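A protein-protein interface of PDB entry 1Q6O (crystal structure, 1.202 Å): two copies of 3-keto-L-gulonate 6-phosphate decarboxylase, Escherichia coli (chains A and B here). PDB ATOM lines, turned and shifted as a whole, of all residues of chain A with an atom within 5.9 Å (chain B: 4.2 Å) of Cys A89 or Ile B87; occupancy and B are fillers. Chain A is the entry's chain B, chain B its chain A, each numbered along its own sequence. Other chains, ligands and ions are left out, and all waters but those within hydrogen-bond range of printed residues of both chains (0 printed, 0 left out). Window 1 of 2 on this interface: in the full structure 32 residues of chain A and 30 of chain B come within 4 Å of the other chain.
Among the printed residues, pairs that only touch across the chains: Cys A89 with Gly B115, Ala A66 with Thr B114, Ile A87 with Cys B89, Ile A87 with Ala B66, Cys A89 with Ile B87, Ile A87 with Ile B87 and Ala A66 with Lys B64.
Of the printed residues of chain B, Cys A89 touches Ile B87 (3.8 Å), Cys B89 (3.2 Å), Thr B114 (3.6 Å), Gly B115 (3.1 Å) and Tyr B116 (2.9 Å).
Ile B87 touches just these residues of chain A: Ile A87 (3.9 Å) and Cys A89 (3.8 Å).
Printed residues of chain B within 4 Å of Thr A114: Cys B89.
Printed residues of chain A within 4 Å of Tyr B116: Cys A89 (2.9 Å).
Of the printed residues of chain B, Ile A87 touches Ala B66 (3.5 Å), Ile B87 (3.9 Å) and Cys B89 (3.5 Å).
Printed residues of chain A within 4 Å of Gly B115: Cys A89 (3.1 Å).
Asp A91 touches none of the printed residues of chain B.
Cys A88 touches none of the printed residues of chain B.
The nearest residue of chain B that does not touch Cys A89 is Cys B88 (4.1 Å).
The nearest residue of chain A that does not touch Ile B87 is Ala A66 (4.1 Å).
The nearest printed residue of chain A that does not touch Tyr B116 is Ala A90 (5.1 Å).
Ala A66 touches Thr B114, but with the chains exchanged Thr A114 does not touch Ala B66 (4.7 Å).
Ile A87 touches its own counterpart, Ile B87.
Cys A89 touches its own counterpart, Cys B89.
Cys A89 touches Thr B114, and with the chains exchanged Thr A114 touches Cys B89.
Positions printed for both chains: 66, 87, 88, 89, 90, 112 and 114.
Of the 11 pairs that touch across the chains among the printed residues, 6 have their exchanged pair printed and touching as well.
The backbone NH of Ile B87 sits at hydrogen-bond distance from the backbone carbonyl oxygen of Ile B65, at 2.9 Å.
SG of Cys B88 lies within hydrogen-bond range of O of Thr B114 (3.5 Å).
The backbone carbonyl oxygen of Tyr B116 is in hydrogen-bond range of the side-chain sulfur of Cys B88 (3.6 Å).
SG of Cys A88 sits at hydrogen-bond distance from O of Thr A114, at 2.8 Å.
Of the 12 printed residues of chain B, 7 touch a printed residue of chain A.
Printed residues of chain B that touch a printed residue of chain A: Lys B64, Ala B66, Ile B87, Cys B89, Thr B114, Gly B115 and Tyr B116.
Hydrophobic or aromatic side chains of chain B within 4 Å of the printed part of chain A: Ala B66, Ile B87 and Tyr B116.
Printed residues of chain A that touch a printed residue of chain B: Ala A66, Ile A87, Cys A89 and Thr A114.
Among the printed residues, 11 pairs touch across the chains.
Among the printed residues, no Asp or Glu carboxylate lies within 4 Å of a Lys or Arg side-chain nitrogen of the other chain.
The backbone carbonyl oxygen (O) of Cys B89 is in hydrogen-bond range of the side-chain hydroxyl (OG1) of Thr A114 (3.2 Å).
SG of Cys A89 lies within hydrogen-bond range of O of Thr B114 (3.6 Å).
O of Cys A89 is in hydrogen-bond range of N of Tyr B116 (2.9 Å).
SG of Cys A89 sits close to SG of Cys B89 (3.2 Å).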
ATOM      1  N   ALA A  66      -2.906 -14.533 -19.190  1.00  0.00           N
ATOM      2  CA  ALA A  66      -3.317 -13.508 -20.158  1.00  0.00           C
ATOM      3  C   ALA A  66      -2.189 -13.075 -21.105  1.00  0.00           C
ATOM      4  O   ALA A  66      -2.461 -12.541 -22.168  1.00  0.00           O
ATOM      5  CB  ALA A  66      -3.816 -12.317 -19.432  1.00  0.00           C
ATOM      6  N   ILE A  87      -6.751 -17.325 -20.368  1.00  0.00           N
ATOM      7  CA  ILE A  87      -7.970 -16.561 -20.566  1.00  0.00           C
ATOM      8  C   ILE A  87      -8.222 -16.293 -22.042  1.00  0.00           C
ATOM      9  O   ILE A  87      -7.283 -16.095 -22.815  1.00  0.00           O
ATOM     10  CB  ILE A  87      -7.959 -15.289 -19.695  1.00  0.00           C
ATOM     11  CG1 ILE A  87      -9.390 -14.774 -19.501  1.00  0.00           C
ATOM     12  CG2 ILE A  87      -7.028 -14.213 -20.253  1.00  0.00           C
ATOM     13  CD1 ILE A  87      -9.511 -13.861 -18.340  1.00  0.00           C
ATOM     14  N   CYS A  88      -9.494 -16.279 -22.430  1.00  0.00           N
ATOM     15  CA  CYS A  88      -9.871 -16.233 -23.846  1.00  0.00           C
ATOM     16  C   CYS A  88      -9.420 -14.984 -24.592  1.00  0.00           C
ATOM     17  O   CYS A  88      -9.230 -15.042 -25.805  1.00  0.00           O
ATOM     18  CB  CYS A  88     -11.397 -16.385 -24.033  1.00  0.00           C
ATOM     19  SG  CYS A  88     -12.351 -15.184 -23.121  1.00  0.00           S
ATOM     20  N   CYS A  89      -9.247 -13.862 -23.906  1.00  0.00           N
ATOM     21  CA  CYS A  89      -8.801 -12.661 -24.610  1.00  0.00           C
ATOM     22  C   CYS A  89      -7.308 -12.635 -24.902  1.00  0.00           C
ATOM     23  O   CYS A  89      -6.860 -11.762 -25.638  1.00  0.00           O
ATOM     24  CB  CYS A  89      -9.221 -11.393 -23.888  1.00  0.00           C
ATOM     25  SG  CYS A  89      -8.400 -11.077 -22.322  1.00  0.00           S
ATOM     26  N   ALA A  90      -6.536 -13.576 -24.385  1.00  0.00           N
ATOM     27  CA  ALA A  90      -5.092 -13.578 -24.591  1.00  0.00           C
ATOM     28  C   ALA A  90      -4.757 -13.615 -26.071  1.00  0.00           C
ATOM     29  O   ALA A  90      -5.455 -14.228 -26.884  1.00  0.00           O
ATOM     30  CB  ALA A  90      -4.443 -14.781 -23.916  1.00  0.00           C
ATOM     31  N   ASP A  91      -3.652 -12.980 -26.424  1.00  0.00           N
ATOM     32  CA  ASP A  91      -3.095 -13.129 -27.767  1.00  0.00           C
ATOM     33  C   ASP A  91      -2.957 -14.616 -28.106  1.00  0.00           C
ATOM     34  O   ASP A  91      -2.583 -15.408 -27.249  1.00  0.00           O
ATOM     35  CB  ASP A  91      -1.729 -12.437 -27.824  1.00  0.00           C
ATOM     36  CG  ASP A  91      -1.184 -12.362 -29.222  1.00  0.00           C
ATOM     37  OD1 ASP A  91      -1.572 -11.416 -29.956  1.00  0.00           O
ATOM     38  OD2 ASP A  91      -0.432 -13.264 -29.613  1.00  0.00           O
ATOM     39  N   GLU A 112     -10.259 -20.363 -20.832  1.00  0.00           N
ATOM     40  CA  GLU A 112     -11.321 -19.875 -19.952  1.00  0.00           C
ATOM     41  C   GLU A 112     -12.157 -18.863 -20.724  1.00  0.00           C
ATOM     42  O   GLU A 112     -11.639 -17.806 -21.119  1.00  0.00           O
ATOM     43  CB  GLU A 112     -10.718 -19.178 -18.731  1.00  0.00           C
ATOM     44  CG  GLU A 112     -11.570 -18.026 -18.129  1.00  0.00           C
ATOM     45  CD  GLU A 112     -12.778 -18.448 -17.309  1.00  0.00           C
ATOM     46  OE1 GLU A 112     -12.853 -19.648 -16.992  1.00  0.00           O
ATOM     47  OE2 GLU A 112     -13.621 -17.539 -16.939  1.00  0.00           O
ATOM     48  N   THR A 114     -14.946 -16.024 -21.393  1.00  0.00           N
ATOM     49  CA  THR A 114     -15.493 -14.813 -20.784  1.00  0.00           C
ATOM     50  C   THR A 114     -15.433 -13.632 -21.782  1.00  0.00           C
ATOM     51  O   THR A 114     -14.695 -13.661 -22.777  1.00  0.00           O
ATOM     52  CB  THR A 114     -14.737 -14.486 -19.445  1.00  0.00           C
ATOM     53  OG1 THR A 114     -15.288 -13.312 -18.840  1.00  0.00           O
ATOM     54  CG2 THR A 114     -13.319 -14.122 -19.664  1.00  0.00           C
ATOM     55  N   TRP A 125      -8.243 -21.137 -31.671  1.00  0.00           N
ATOM     56  CA  TRP A 125      -7.814 -22.025 -30.593  1.00  0.00           C
ATOM     57  C   TRP A 125      -7.768 -23.437 -31.116  1.00  0.00           C
ATOM     58  O   TRP A 125      -6.805 -24.137 -30.866  1.00  0.00           O
ATOM     59  CB  TRP A 125      -8.709 -21.966 -29.344  1.00  0.00           C
ATOM     60  CG  TRP A 125      -8.846 -20.598 -28.770  1.00  0.00           C
ATOM     61  CD1 TRP A 125      -7.874 -19.638 -28.692  1.00  0.00           C
ATOM     62  CD2 TRP A 125     -10.035 -20.016 -28.229  1.00  0.00           C
ATOM     63  NE1 TRP A 125      -8.398 -18.497 -28.146  1.00  0.00           N
ATOM     64  CE2 TRP A 125      -9.725 -18.697 -27.859  1.00  0.00           C
ATOM     65  CE3 TRP A 125     -11.337 -20.488 -27.998  1.00  0.00           C
ATOM     66  CZ2 TRP A 125     -10.664 -17.842 -27.291  1.00  0.00           C
ATOM     67  CZ3 TRP A 125     -12.278 -19.639 -27.482  1.00  0.00           C
ATOM     68  CH2 TRP A 125     -11.944 -18.328 -27.119  1.00  0.00           C
ATOM     69  N   LYS B  64      -4.679  -8.718 -12.845  1.00  0.00           N
ATOM     70  CA  LYS B  64      -5.478  -9.046 -14.036  1.00  0.00           C
ATOM     71  C   LYS B  64      -6.762  -9.794 -13.644  1.00  0.00           C
ATOM     72  O   LYS B  64      -7.126 -10.819 -14.212  1.00  0.00           O
ATOM     73  CB  LYS B  64      -4.667  -9.797 -15.096  1.00  0.00           C
ATOM     74  CG  LYS B  64      -3.549  -8.949 -15.690  1.00  0.00           C
ATOM     75  CD  LYS B  64      -2.740  -9.731 -16.720  1.00  0.00           C
ATOM     76  CE  LYS B  64      -1.746  -8.882 -17.482  1.00  0.00           C
ATOM     77  NZ  LYS B  64      -0.767  -8.264 -16.578  1.00  0.00           N
ATOM     78  N   ILE B  65      -7.454  -9.232 -12.674  1.00  0.00           N
ATOM     79  CA  ILE B  65      -8.657  -9.839 -12.116  1.00  0.00           C
ATOM     80  C   ILE B  65      -9.684 -10.070 -13.222  1.00  0.00           C
ATOM     81  O   ILE B  65     -10.027  -9.148 -13.963  1.00  0.00           O
ATOM     82  CB  ILE B  65      -9.245  -8.923 -11.026  1.00  0.00           C
ATOM     83  CG1 ILE B  65      -8.284  -8.822  -9.839  1.00  0.00           C
ATOM     84  CG2 ILE B  65     -10.631  -9.415 -10.588  1.00  0.00           C
ATOM     85  CD1 ILE B  65      -8.617  -7.753  -8.857  1.00  0.00           C
ATOM     86  N   ALA B  66     -10.198 -11.297 -13.284  1.00  0.00           N
ATOM     87  CA  ALA B  66     -11.091 -11.709 -14.367  1.00  0.00           C
ATOM     88  C   ALA B  66     -12.516 -11.971 -13.939  1.00  0.00           C
ATOM     89  O   ALA B  66     -13.413 -11.920 -14.779  1.00  0.00           O
ATOM     90  CB  ALA B  66     -10.545 -12.936 -15.077  1.00  0.00           C
ATOM     91  N   VAL B  86      -7.652  -5.127 -13.627  1.00  0.00           N
ATOM     92  CA  VAL B  86      -8.783  -5.965 -14.005  1.00  0.00           C
ATOM     93  C   VAL B  86      -8.634  -6.223 -15.497  1.00  0.00           C
ATOM     94  O   VAL B  86      -8.462  -5.277 -16.270  1.00  0.00           O
ATOM     95  CB  VAL B  86     -10.130  -5.276 -13.691  1.00  0.00           C
ATOM     96  CG1 VAL B  86     -11.297  -6.021 -14.329  1.00  0.00           C
ATOM     97  CG2 VAL B  86     -10.340  -5.148 -12.207  1.00  0.00           C
ATOM     98  N   ILE B  87      -8.649  -7.463 -15.914  1.00  0.00           N
ATOM     99  CA  ILE B  87      -8.445  -7.765 -17.331  1.00  0.00           C
ATOM    100  C   ILE B  87      -9.651  -7.295 -18.162  1.00  0.00           C
ATOM    101  O   ILE B  87     -10.801  -7.346 -17.728  1.00  0.00           O
ATOM    102  CB  ILE B  87      -8.164  -9.273 -17.540  1.00  0.00           C
ATOM    103  CG1 ILE B  87      -7.619  -9.568 -18.936  1.00  0.00           C
ATOM    104  CG2 ILE B  87      -9.392 -10.135 -17.264  1.00  0.00           C
ATOM    105  CD1 ILE B  87      -6.241  -9.075 -19.229  1.00  0.00           C
ATOM    106  N   CYS B  88      -9.360  -6.857 -19.381  1.00  0.00           N
ATOM    107  CA  CYS B  88     -10.356  -6.240 -20.253  1.00  0.00           C
ATOM    108  C   CYS B  88     -11.558  -7.132 -20.569  1.00  0.00           C
ATOM    109  O   CYS B  88     -12.643  -6.612 -20.781  1.00  0.00           O
ATOM    110  CB  CYS B  88      -9.684  -5.754 -21.546  1.00  0.00           C
ATOM    111  SG  CYS B  88      -8.668  -6.979 -22.406  1.00  0.00           S
ATOM    112  N   CYS B  89     -11.398  -8.448 -20.586  1.00  0.00           N
ATOM    113  CA  CYS B  89     -12.513  -9.305 -20.940  1.00  0.00           C
ATOM    114  C   CYS B  89     -13.391  -9.685 -19.744  1.00  0.00           C
ATOM    115  O   CYS B  89     -14.359 -10.421 -19.901  1.00  0.00           O
ATOM    116  CB  CYS B  89     -12.035 -10.553 -21.653  1.00  0.00           C
ATOM    117  SG  CYS B  89     -11.048 -11.664 -20.657  1.00  0.00           S
ATOM    118  N   ALA B  90     -13.100  -9.170 -18.559  1.00  0.00           N
ATOM    119  CA  ALA B  90     -13.931  -9.423 -17.397  1.00  0.00           C
ATOM    120  C   ALA B  90     -15.345  -8.888 -17.662  1.00  0.00           C
ATOM    121  O   ALA B  90     -15.545  -7.880 -18.319  1.00  0.00           O
ATOM    122  CB  ALA B  90     -13.358  -8.738 -16.191  1.00  0.00           C
ATOM    123  N   GLU B 112      -6.815  -3.606 -17.789  1.00  0.00           N
ATOM    124  CA  GLU B 112      -5.661  -4.077 -18.501  1.00  0.00           C
ATOM    125  C   GLU B 112      -6.087  -4.484 -19.906  1.00  0.00           C
ATOM    126  O   GLU B 112      -6.825  -5.450 -20.096  1.00  0.00           O
ATOM    127  CB  GLU B 112      -5.062  -5.266 -17.723  1.00  0.00           C
ATOM    128  CG  GLU B 112      -3.705  -4.958 -17.103  1.00  0.00           C
ATOM    129  CD  GLU B 112      -2.603  -4.863 -18.133  1.00  0.00           C
ATOM    130  OE1 GLU B 112      -2.878  -5.182 -19.294  1.00  0.00           O
ATOM    131  OE2 GLU B 112      -1.451  -4.474 -17.795  1.00  0.00           O
ATOM    132  N   THR B 114      -4.892  -6.132 -22.360  1.00  0.00           N
ATOM    133  CA  THR B 114      -3.983  -7.194 -22.744  1.00  0.00           C
ATOM    134  C   THR B 114      -4.841  -8.144 -23.575  1.00  0.00           C
ATOM    135  O   THR B 114      -5.772  -8.751 -23.055  1.00  0.00           O
ATOM    136  CB  THR B 114      -3.421  -7.892 -21.473  1.00  0.00           C
ATOM    137  OG1 THR B 114      -2.505  -7.018 -20.749  1.00  0.00           O
ATOM    138  CG2 THR B 114      -2.623  -9.154 -21.839  1.00  0.00           C
ATOM    139  N   GLY B 115      -4.544  -8.238 -24.871  1.00  0.00           N
ATOM    140  CA  GLY B 115      -5.300  -9.071 -25.791  1.00  0.00           C
ATOM    141  C   GLY B 115      -6.496  -8.345 -26.389  1.00  0.00           C
ATOM    142  O   GLY B 115      -6.456  -7.134 -26.623  1.00  0.00           O
ATOM    143  N   TYR B 116      -7.558  -9.097 -26.661  1.00  0.00           N
ATOM    144  CA  TYR B 116      -8.734  -8.626 -27.396  1.00  0.00           C
ATOM    145  C   TYR B 116      -9.740  -7.884 -26.516  1.00  0.00           C
ATOM    146  O   TYR B 116     -10.107  -8.376 -25.438  1.00  0.00           O
ATOM    147  CB  TYR B 116      -9.433  -9.845 -28.019  1.00  0.00           C
ATOM    148  CG  TYR B 116     -10.725  -9.540 -28.732  1.00  0.00           C
ATOM    149  CD1 TYR B 116     -10.703  -9.024 -30.014  1.00  0.00           C
ATOM    150  CD2 TYR B 116     -11.963  -9.772 -28.134  1.00  0.00           C
ATOM    151  CE1 TYR B 116     -11.872  -8.746 -30.695  1.00  0.00           C
ATOM    152  CE2 TYR B 116     -13.149  -9.490 -28.817  1.00  0.00           C
ATOM    153  CZ  TYR B 116     -13.082  -8.971 -30.095  1.00  0.00           C
ATOM    154  OH  TYR B 116     -14.237  -8.692 -30.789  1.00  0.00           O
